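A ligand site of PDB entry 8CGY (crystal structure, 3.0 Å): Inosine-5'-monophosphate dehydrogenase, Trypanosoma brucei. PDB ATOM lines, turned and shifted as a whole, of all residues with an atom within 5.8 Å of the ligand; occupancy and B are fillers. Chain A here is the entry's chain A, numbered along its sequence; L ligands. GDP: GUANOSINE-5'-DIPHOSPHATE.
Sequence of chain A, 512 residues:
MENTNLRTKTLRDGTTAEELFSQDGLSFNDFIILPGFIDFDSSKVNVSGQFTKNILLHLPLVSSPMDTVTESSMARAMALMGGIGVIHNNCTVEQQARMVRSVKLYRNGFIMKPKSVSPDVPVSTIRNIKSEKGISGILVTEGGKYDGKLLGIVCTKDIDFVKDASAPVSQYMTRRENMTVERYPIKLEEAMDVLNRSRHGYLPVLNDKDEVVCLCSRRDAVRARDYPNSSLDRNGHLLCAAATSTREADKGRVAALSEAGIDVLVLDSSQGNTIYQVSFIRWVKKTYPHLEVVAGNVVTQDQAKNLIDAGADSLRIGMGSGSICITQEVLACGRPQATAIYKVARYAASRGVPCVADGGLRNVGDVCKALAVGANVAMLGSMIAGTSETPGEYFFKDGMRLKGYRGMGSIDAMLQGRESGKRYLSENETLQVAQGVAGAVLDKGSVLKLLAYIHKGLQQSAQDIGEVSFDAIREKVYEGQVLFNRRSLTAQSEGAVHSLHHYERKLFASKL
The backbone carbonyl oxygen of Ser 136 lies within hydrogen-bond range of a nitrogen (N1) of the ligand (3.1 Å).
The backbone carbonyl oxygen (O) of Lys 113 lies within hydrogen-bond range of an oxygen (O3') of the ligand, at 3.0 Å.
O2A of the ligand is in salt-bridge range of NZ of Lys 133 (2.8 Å).
The backbone carbonyl oxygen (O) of Lys 115 is in hydrogen-bond range of a nitrogen (N2) of the ligand, 3.1 Å away.
O of Gly 137 sits at hydrogen-bond distance from N2 of the ligand (2.8 Å).
NZ of Lys 115 lies within salt-bridge range of O2A of the ligand (2.7 Å).
A nitrogen (N3) of the ligand lies within hydrogen-bond range of the backbone NH of Lys 115 (2.9 Å).
The guanidinium group (NH2) of Arg 101 lies within salt-bridge range of an oxygen (O1B) of the ligand (3.3 Å).
The backbone carbonyl oxygen of Leu 215 sits at hydrogen-bond distance from the backbone NH of Ile 111.
The backbone carbonyl oxygen of Lys 115 lies within hydrogen-bond range of the backbone NH of Leu 139 (3.1 Å).
Merely in contact with the ligand: Ile 135, Leu 105, Pro 114, Arg 98, Ile 111, Leu 215, Tyr 202, Ile 138 and Leu 139.
Within 4 Å of the ligand: Arg 98, Arg 101, Leu 105, Ile 111, Lys 113, Pro 114, Lys 115, Lys 133, Ile 135, Ser 136, Gly 137, Ile 138, Leu 139, Tyr 202 and Leu 215.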
ATOM      1  N   ARG A  98     -25.388  -1.560  -1.513  1.00  0.00           N
ATOM      2  CA  ARG A  98     -24.175  -1.912  -0.777  1.00  0.00           C
ATOM      3  C   ARG A  98     -23.457  -0.665  -0.284  1.00  0.00           C
ATOM      4  O   ARG A  98     -22.991  -0.616   0.861  1.00  0.00           O
ATOM      5  CB  ARG A  98     -23.262  -2.764  -1.665  1.00  0.00           C
ATOM      6  CG  ARG A  98     -22.249  -3.616  -0.884  1.00  0.00           C
ATOM      7  CD  ARG A  98     -21.702  -4.800  -1.697  1.00  0.00           C
ATOM      8  NE  ARG A  98     -21.003  -4.386  -2.914  1.00  0.00           N
ATOM      9  CZ  ARG A  98     -21.415  -4.653  -4.146  1.00  0.00           C
ATOM     10  NH1 ARG A  98     -22.502  -5.366  -4.377  1.00  0.00           N
ATOM     11  NH2 ARG A  98     -20.701  -4.200  -5.177  1.00  0.00           N
ATOM     12  N   ARG A 101     -25.214   0.566   2.831  1.00  0.00           N
ATOM     13  CA  ARG A 101     -24.885  -0.210   4.023  1.00  0.00           C
ATOM     14  C   ARG A 101     -23.479   0.134   4.518  1.00  0.00           C
ATOM     15  O   ARG A 101     -23.253   0.204   5.739  1.00  0.00           O
ATOM     16  CB  ARG A 101     -25.007  -1.710   3.743  1.00  0.00           C
ATOM     17  CG  ARG A 101     -26.419  -2.155   3.362  1.00  0.00           C
ATOM     18  CD  ARG A 101     -26.617  -3.657   3.514  1.00  0.00           C
ATOM     19  NE  ARG A 101     -25.591  -4.421   2.831  1.00  0.00           N
ATOM     20  CZ  ARG A 101     -25.648  -4.792   1.560  1.00  0.00           C
ATOM     21  NH1 ARG A 101     -26.678  -4.471   0.793  1.00  0.00           N
ATOM     22  NH2 ARG A 101     -24.652  -5.493   1.037  1.00  0.00           N
ATOM     23  N   LEU A 105     -23.611   1.175   8.316  1.00  0.00           N
ATOM     24  CA  LEU A 105     -23.010   0.248   9.266  1.00  0.00           C
ATOM     25  C   LEU A 105     -21.611   0.648   9.703  1.00  0.00           C
ATOM     26  O   LEU A 105     -21.011  -0.070  10.513  1.00  0.00           O
ATOM     27  CB  LEU A 105     -22.984  -1.164   8.675  1.00  0.00           C
ATOM     28  CG  LEU A 105     -24.366  -1.775   8.426  1.00  0.00           C
ATOM     29  CD1 LEU A 105     -24.242  -3.079   7.646  1.00  0.00           C
ATOM     30  CD2 LEU A 105     -25.115  -1.997   9.744  1.00  0.00           C
ATOM     31  N   TYR A 106     -21.070   1.753   9.201  1.00  0.00           N
ATOM     32  CA  TYR A 106     -19.741   2.203   9.604  1.00  0.00           C
ATOM     33  C   TYR A 106     -19.702   2.546  11.085  1.00  0.00           C
ATOM     34  O   TYR A 106     -18.976   1.926  11.866  1.00  0.00           O
ATOM     35  CB  TYR A 106     -19.307   3.402   8.749  1.00  0.00           C
ATOM     36  CG  TYR A 106     -18.022   4.048   9.199  1.00  0.00           C
ATOM     37  CD1 TYR A 106     -16.788   3.481   8.915  1.00  0.00           C
ATOM     38  CD2 TYR A 106     -18.045   5.242   9.917  1.00  0.00           C
ATOM     39  CE1 TYR A 106     -15.608   4.084   9.318  1.00  0.00           C
ATOM     40  CE2 TYR A 106     -16.870   5.857  10.324  1.00  0.00           C
ATOM     41  CZ  TYR A 106     -15.659   5.270  10.030  1.00  0.00           C
ATOM     42  OH  TYR A 106     -14.489   5.877  10.436  1.00  0.00           O
ATOM     43  N   ASN A 108     -21.709   2.625  14.639  1.00  0.00           N
ATOM     44  CA  ASN A 108     -22.855   2.180  15.420  1.00  0.00           C
ATOM     45  C   ASN A 108     -22.409   1.914  16.843  1.00  0.00           C
ATOM     46  O   ASN A 108     -21.208   1.790  17.128  1.00  0.00           O
ATOM     47  CB  ASN A 108     -23.536   0.951  14.815  1.00  0.00           C
ATOM     48  CG  ASN A 108     -22.553  -0.035  14.196  1.00  0.00           C
ATOM     49  OD1 ASN A 108     -21.341   0.125  14.314  1.00  0.00           O
ATOM     50  ND2 ASN A 108     -23.077  -1.056  13.539  1.00  0.00           N
ATOM     51  N   ILE A 111     -22.919  -3.420  17.395  1.00  0.00           N
ATOM     52  CA  ILE A 111     -22.812  -4.023  16.069  1.00  0.00           C
ATOM     53  C   ILE A 111     -23.700  -5.266  16.064  1.00  0.00           C
ATOM     54  O   ILE A 111     -23.424  -6.239  16.776  1.00  0.00           O
ATOM     55  CB  ILE A 111     -21.361  -4.363  15.712  1.00  0.00           C
ATOM     56  CG1 ILE A 111     -20.502  -3.106  15.813  1.00  0.00           C
ATOM     57  CG2 ILE A 111     -21.282  -4.930  14.296  1.00  0.00           C
ATOM     58  CD1 ILE A 111     -19.032  -3.368  15.670  1.00  0.00           C
ATOM     59  N   MET A 112     -24.770  -5.227  15.281  1.00  0.00           N
ATOM     60  CA  MET A 112     -25.781  -6.273  15.363  1.00  0.00           C
ATOM     61  C   MET A 112     -25.400  -7.514  14.578  1.00  0.00           C
ATOM     62  O   MET A 112     -25.701  -8.629  15.018  1.00  0.00           O
ATOM     63  CB  MET A 112     -27.132  -5.729  14.899  1.00  0.00           C
ATOM     64  CG  MET A 112     -27.800  -4.858  15.931  1.00  0.00           C
ATOM     65  SD  MET A 112     -27.601  -5.536  17.602  1.00  0.00           S
ATOM     66  CE  MET A 112     -28.204  -7.209  17.390  1.00  0.00           C
ATOM     67  N   LYS A 113     -24.717  -7.359  13.451  1.00  0.00           N
ATOM     68  CA  LYS A 113     -24.299  -8.476  12.611  1.00  0.00           C
ATOM     69  C   LYS A 113     -22.785  -8.408  12.432  1.00  0.00           C
ATOM     70  O   LYS A 113     -22.287  -8.099  11.335  1.00  0.00           O
ATOM     71  CB  LYS A 113     -25.007  -8.459  11.257  1.00  0.00           C
ATOM     72  CG  LYS A 113     -26.495  -8.775  11.338  1.00  0.00           C
ATOM     73  CD  LYS A 113     -27.148  -8.727   9.967  1.00  0.00           C
ATOM     74  CE  LYS A 113     -28.647  -8.993  10.052  1.00  0.00           C
ATOM     75  NZ  LYS A 113     -29.295  -8.884   8.716  1.00  0.00           N
ATOM     76  N   PRO A 114     -22.021  -8.677  13.489  1.00  0.00           N
ATOM     77  CA  PRO A 114     -20.562  -8.591  13.391  1.00  0.00           C
ATOM     78  C   PRO A 114     -20.017  -9.532  12.330  1.00  0.00           C
ATOM     79  O   PRO A 114     -20.420 -10.688  12.215  1.00  0.00           O
ATOM     80  CB  PRO A 114     -20.075  -8.975  14.786  1.00  0.00           C
ATOM     81  CG  PRO A 114     -21.221  -9.705  15.413  1.00  0.00           C
ATOM     82  CD  PRO A 114     -22.456  -9.070  14.836  1.00  0.00           C
ATOM     83  N   LYS A 115     -19.058  -9.017  11.550  1.00  0.00           N
ATOM     84  CA  LYS A 115     -18.389  -9.822  10.533  1.00  0.00           C
ATOM     85  C   LYS A 115     -17.736 -11.031  11.179  1.00  0.00           C
ATOM     86  O   LYS A 115     -16.911 -10.896  12.087  1.00  0.00           O
ATOM     87  CB  LYS A 115     -17.357  -8.979   9.803  1.00  0.00           C
ATOM     88  CG  LYS A 115     -16.662  -9.691   8.644  1.00  0.00           C
ATOM     89  CD  LYS A 115     -17.562  -9.818   7.418  1.00  0.00           C
ATOM     90  CE  LYS A 115     -16.736  -9.861   6.134  1.00  0.00           C
ATOM     91  NZ  LYS A 115     -17.531  -9.590   4.894  1.00  0.00           N
ATOM     92  N   SER A 116     -18.106 -12.217  10.710  1.00  0.00           N
ATOM     93  CA  SER A 116     -17.659 -13.472  11.290  1.00  0.00           C
ATOM     94  C   SER A 116     -17.084 -14.381  10.208  1.00  0.00           C
ATOM     95  O   SER A 116     -17.432 -14.270   9.030  1.00  0.00           O
ATOM     96  CB  SER A 116     -18.820 -14.183  12.010  1.00  0.00           C
ATOM     97  OG  SER A 116     -20.008 -14.110  11.243  1.00  0.00           O
ATOM     98  N   LYS A 133     -12.854  -3.637   3.297  1.00  0.00           N
ATOM     99  CA  LYS A 133     -13.939  -3.106   4.108  1.00  0.00           C
ATOM    100  C   LYS A 133     -13.452  -2.324   5.319  1.00  0.00           C
ATOM    101  O   LYS A 133     -14.263  -1.639   5.961  1.00  0.00           O
ATOM    102  CB  LYS A 133     -14.859  -4.250   4.536  1.00  0.00           C
ATOM    103  CG  LYS A 133     -15.689  -4.848   3.391  1.00  0.00           C
ATOM    104  CD  LYS A 133     -16.696  -5.877   3.880  1.00  0.00           C
ATOM    105  CE  LYS A 133     -17.628  -6.351   2.780  1.00  0.00           C
ATOM    106  NZ  LYS A 133     -18.580  -7.376   3.287  1.00  0.00           N
ATOM    107  N   ILE A 135     -12.347  -3.302   8.290  1.00  0.00           N
ATOM    108  CA  ILE A 135     -12.929  -3.843   9.511  1.00  0.00           C
ATOM    109  C   ILE A 135     -11.915  -4.780  10.144  1.00  0.00           C
ATOM    110  O   ILE A 135     -11.461  -5.735   9.493  1.00  0.00           O
ATOM    111  CB  ILE A 135     -14.257  -4.566   9.232  1.00  0.00           C
ATOM    112  CG1 ILE A 135     -15.146  -3.705   8.337  1.00  0.00           C
ATOM    113  CG2 ILE A 135     -14.990  -4.883  10.522  1.00  0.00           C
ATOM    114  CD1 ILE A 135     -16.323  -4.455   7.739  1.00  0.00           C
ATOM    115  N   SER A 136     -11.527  -4.489  11.377  1.00  0.00           N
ATOM    116  CA  SER A 136     -10.695  -5.379  12.183  1.00  0.00           C
ATOM    117  C   SER A 136     -11.593  -6.168  13.125  1.00  0.00           C
ATOM    118  O   SER A 136     -12.832  -6.157  13.002  1.00  0.00           O
ATOM    119  CB  SER A 136      -9.622  -4.574  12.936  1.00  0.00           C
ATOM    120  OG  SER A 136      -8.745  -5.410  13.670  1.00  0.00           O
ATOM    121  N   GLY A 137     -10.997  -6.879  14.076  1.00  0.00           N
ATOM    122  CA  GLY A 137     -11.791  -7.527  15.100  1.00  0.00           C
ATOM    123  C   GLY A 137     -12.771  -8.549  14.557  1.00  0.00           C
ATOM    124  O   GLY A 137     -13.926  -8.589  14.993  1.00  0.00           O
ATOM    125  N   ILE A 138     -12.328  -9.374  13.613  1.00  0.00           N
ATOM    126  CA  ILE A 138     -13.195 -10.390  13.022  1.00  0.00           C
ATOM    127  C   ILE A 138     -13.531 -11.447  14.067  1.00  0.00           C
ATOM    128  O   ILE A 138     -12.641 -11.949  14.772  1.00  0.00           O
ATOM    129  CB  ILE A 138     -12.517 -11.007  11.794  1.00  0.00           C
ATOM    130  CG1 ILE A 138     -12.055  -9.900  10.846  1.00  0.00           C
ATOM    131  CG2 ILE A 138     -13.452 -11.988  11.101  1.00  0.00           C
ATOM    132  CD1 ILE A 138     -13.028  -8.754  10.740  1.00  0.00           C
ATOM    133  N   LEU A 139     -14.812 -11.792  14.185  1.00  0.00           N
ATOM    134  CA  LEU A 139     -15.246 -12.820  15.113  1.00  0.00           C
ATOM    135  C   LEU A 139     -15.182 -14.186  14.439  1.00  0.00           C
ATOM    136  O   LEU A 139     -15.745 -14.374  13.359  1.00  0.00           O
ATOM    137  CB  LEU A 139     -16.659 -12.539  15.617  1.00  0.00           C
ATOM    138  CG  LEU A 139     -16.819 -11.323  16.533  1.00  0.00           C
ATOM    139  CD1 LEU A 139     -18.202 -11.294  17.148  1.00  0.00           C
ATOM    140  CD2 LEU A 139     -15.758 -11.314  17.615  1.00  0.00           C
ATOM    141  N   TYR A 202     -12.346  -4.672  21.357  1.00  0.00           N
ATOM    142  CA  TYR A 202     -13.631  -5.279  21.053  1.00  0.00           C
ATOM    143  C   TYR A 202     -14.176  -5.996  22.275  1.00  0.00           C
ATOM    144  O   TYR A 202     -13.425  -6.500  23.109  1.00  0.00           O
ATOM    145  CB  TYR A 202     -13.505  -6.207  19.835  1.00  0.00           C
ATOM    146  CG  TYR A 202     -13.001  -5.438  18.625  1.00  0.00           C
ATOM    147  CD1 TYR A 202     -13.855  -4.585  17.932  1.00  0.00           C
ATOM    148  CD2 TYR A 202     -11.688  -5.522  18.205  1.00  0.00           C
ATOM    149  CE1 TYR A 202     -13.416  -3.854  16.846  1.00  0.00           C
ATOM    150  CE2 TYR A 202     -11.232  -4.799  17.113  1.00  0.00           C
ATOM    151  CZ  TYR A 202     -12.104  -3.974  16.439  1.00  0.00           C
ATOM    152  OH  TYR A 202     -11.660  -3.256  15.348  1.00  0.00           O
ATOM    153  N   LEU A 215     -21.776  -6.969  19.080  1.00  0.00           N
ATOM    154  CA  LEU A 215     -20.375  -6.662  19.346  1.00  0.00           C
ATOM    155  C   LEU A 215     -20.211  -5.168  19.592  1.00  0.00           C
ATOM    156  O   LEU A 215     -20.889  -4.344  18.975  1.00  0.00           O
ATOM    157  CB  LEU A 215     -19.499  -7.114  18.172  1.00  0.00           C
ATOM    158  CG  LEU A 215     -18.020  -6.737  18.182  1.00  0.00           C
ATOM    159  CD1 LEU A 215     -17.365  -7.182  19.478  1.00  0.00           C
ATOM    160  CD2 LEU A 215     -17.321  -7.370  16.998  1.00  0.00           C
ATOM    161  N   SER A 217     -17.342  -2.023  19.692  1.00  0.00           N
ATOM    162  CA  SER A 217     -16.077  -1.635  19.091  1.00  0.00           C
ATOM    163  C   SER A 217     -15.551  -0.384  19.781  1.00  0.00           C
ATOM    164  O   SER A 217     -16.277   0.597  19.934  1.00  0.00           O
ATOM    165  CB  SER A 217     -16.265  -1.397  17.586  1.00  0.00           C
ATOM    166  OG  SER A 217     -15.357  -0.448  17.050  1.00  0.00           O
HETATM  167  PB  GDP L   1     -21.685  -7.702   2.445  1.00  0.00           P
HETATM  168  O1B GDP L   1     -23.166  -7.995   2.678  1.00  0.00           O
HETATM  169  O2B GDP L   1     -21.542  -6.893   1.176  1.00  0.00           O
HETATM  170  O3B GDP L   1     -20.913  -8.986   2.292  1.00  0.00           O
HETATM  171  O3A GDP L   1     -21.087  -6.816   3.738  1.00  0.00           O
HETATM  172  PA  GDP L   1     -20.887  -7.350   5.327  1.00  0.00           P
HETATM  173  O1A GDP L   1     -22.213  -7.710   5.950  1.00  0.00           O
HETATM  174  O2A GDP L   1     -19.970  -8.560   5.357  1.00  0.00           O
HETATM  175  O5' GDP L   1     -20.244  -6.086   6.171  1.00  0.00           O
HETATM  176  C5' GDP L   1     -19.600  -6.247   7.400  1.00  0.00           C
HETATM  177  C4' GDP L   1     -20.544  -6.431   8.543  1.00  0.00           C
HETATM  178  O4' GDP L   1     -19.587  -6.286   9.938  1.00  0.00           O
HETATM  179  C3' GDP L   1     -21.480  -5.542   8.641  1.00  0.00           C
HETATM  180  O3' GDP L   1     -22.721  -6.215   9.093  1.00  0.00           O
HETATM  181  C2' GDP L   1     -21.023  -4.515   9.717  1.00  0.00           C
HETATM  182  O2' GDP L   1     -22.017  -4.028  10.421  1.00  0.00           O
HETATM  183  C1' GDP L   1     -20.122  -5.371  10.705  1.00  0.00           C
HETATM  184  N9  GDP L   1     -19.086  -4.605  11.374  1.00  0.00           N
HETATM  185  C8  GDP L   1     -18.933  -3.301  11.376  1.00  0.00           C
HETATM  186  N7  GDP L   1     -17.875  -2.982  12.121  1.00  0.00           N
HETATM  187  C5  GDP L   1     -17.347  -4.118  12.583  1.00  0.00           C
HETATM  188  C6  GDP L   1     -16.153  -4.399  13.468  1.00  0.00           C
HETATM  189  O6  GDP L   1     -15.501  -3.500  13.862  1.00  0.00           O
HETATM  190  N1  GDP L   1     -15.831  -5.766  13.809  1.00  0.00           N
HETATM  191  C2  GDP L   1     -16.659  -6.845  13.310  1.00  0.00           C
HETATM  192  N2  GDP L   1     -16.361  -8.233  13.641  1.00  0.00           N
HETATM  193  N3  GDP L   1     -17.813  -6.554  12.460  1.00  0.00           N
HETATM  194  C4  GDP L   1     -18.129  -5.145  12.117  1.00  0.00           C
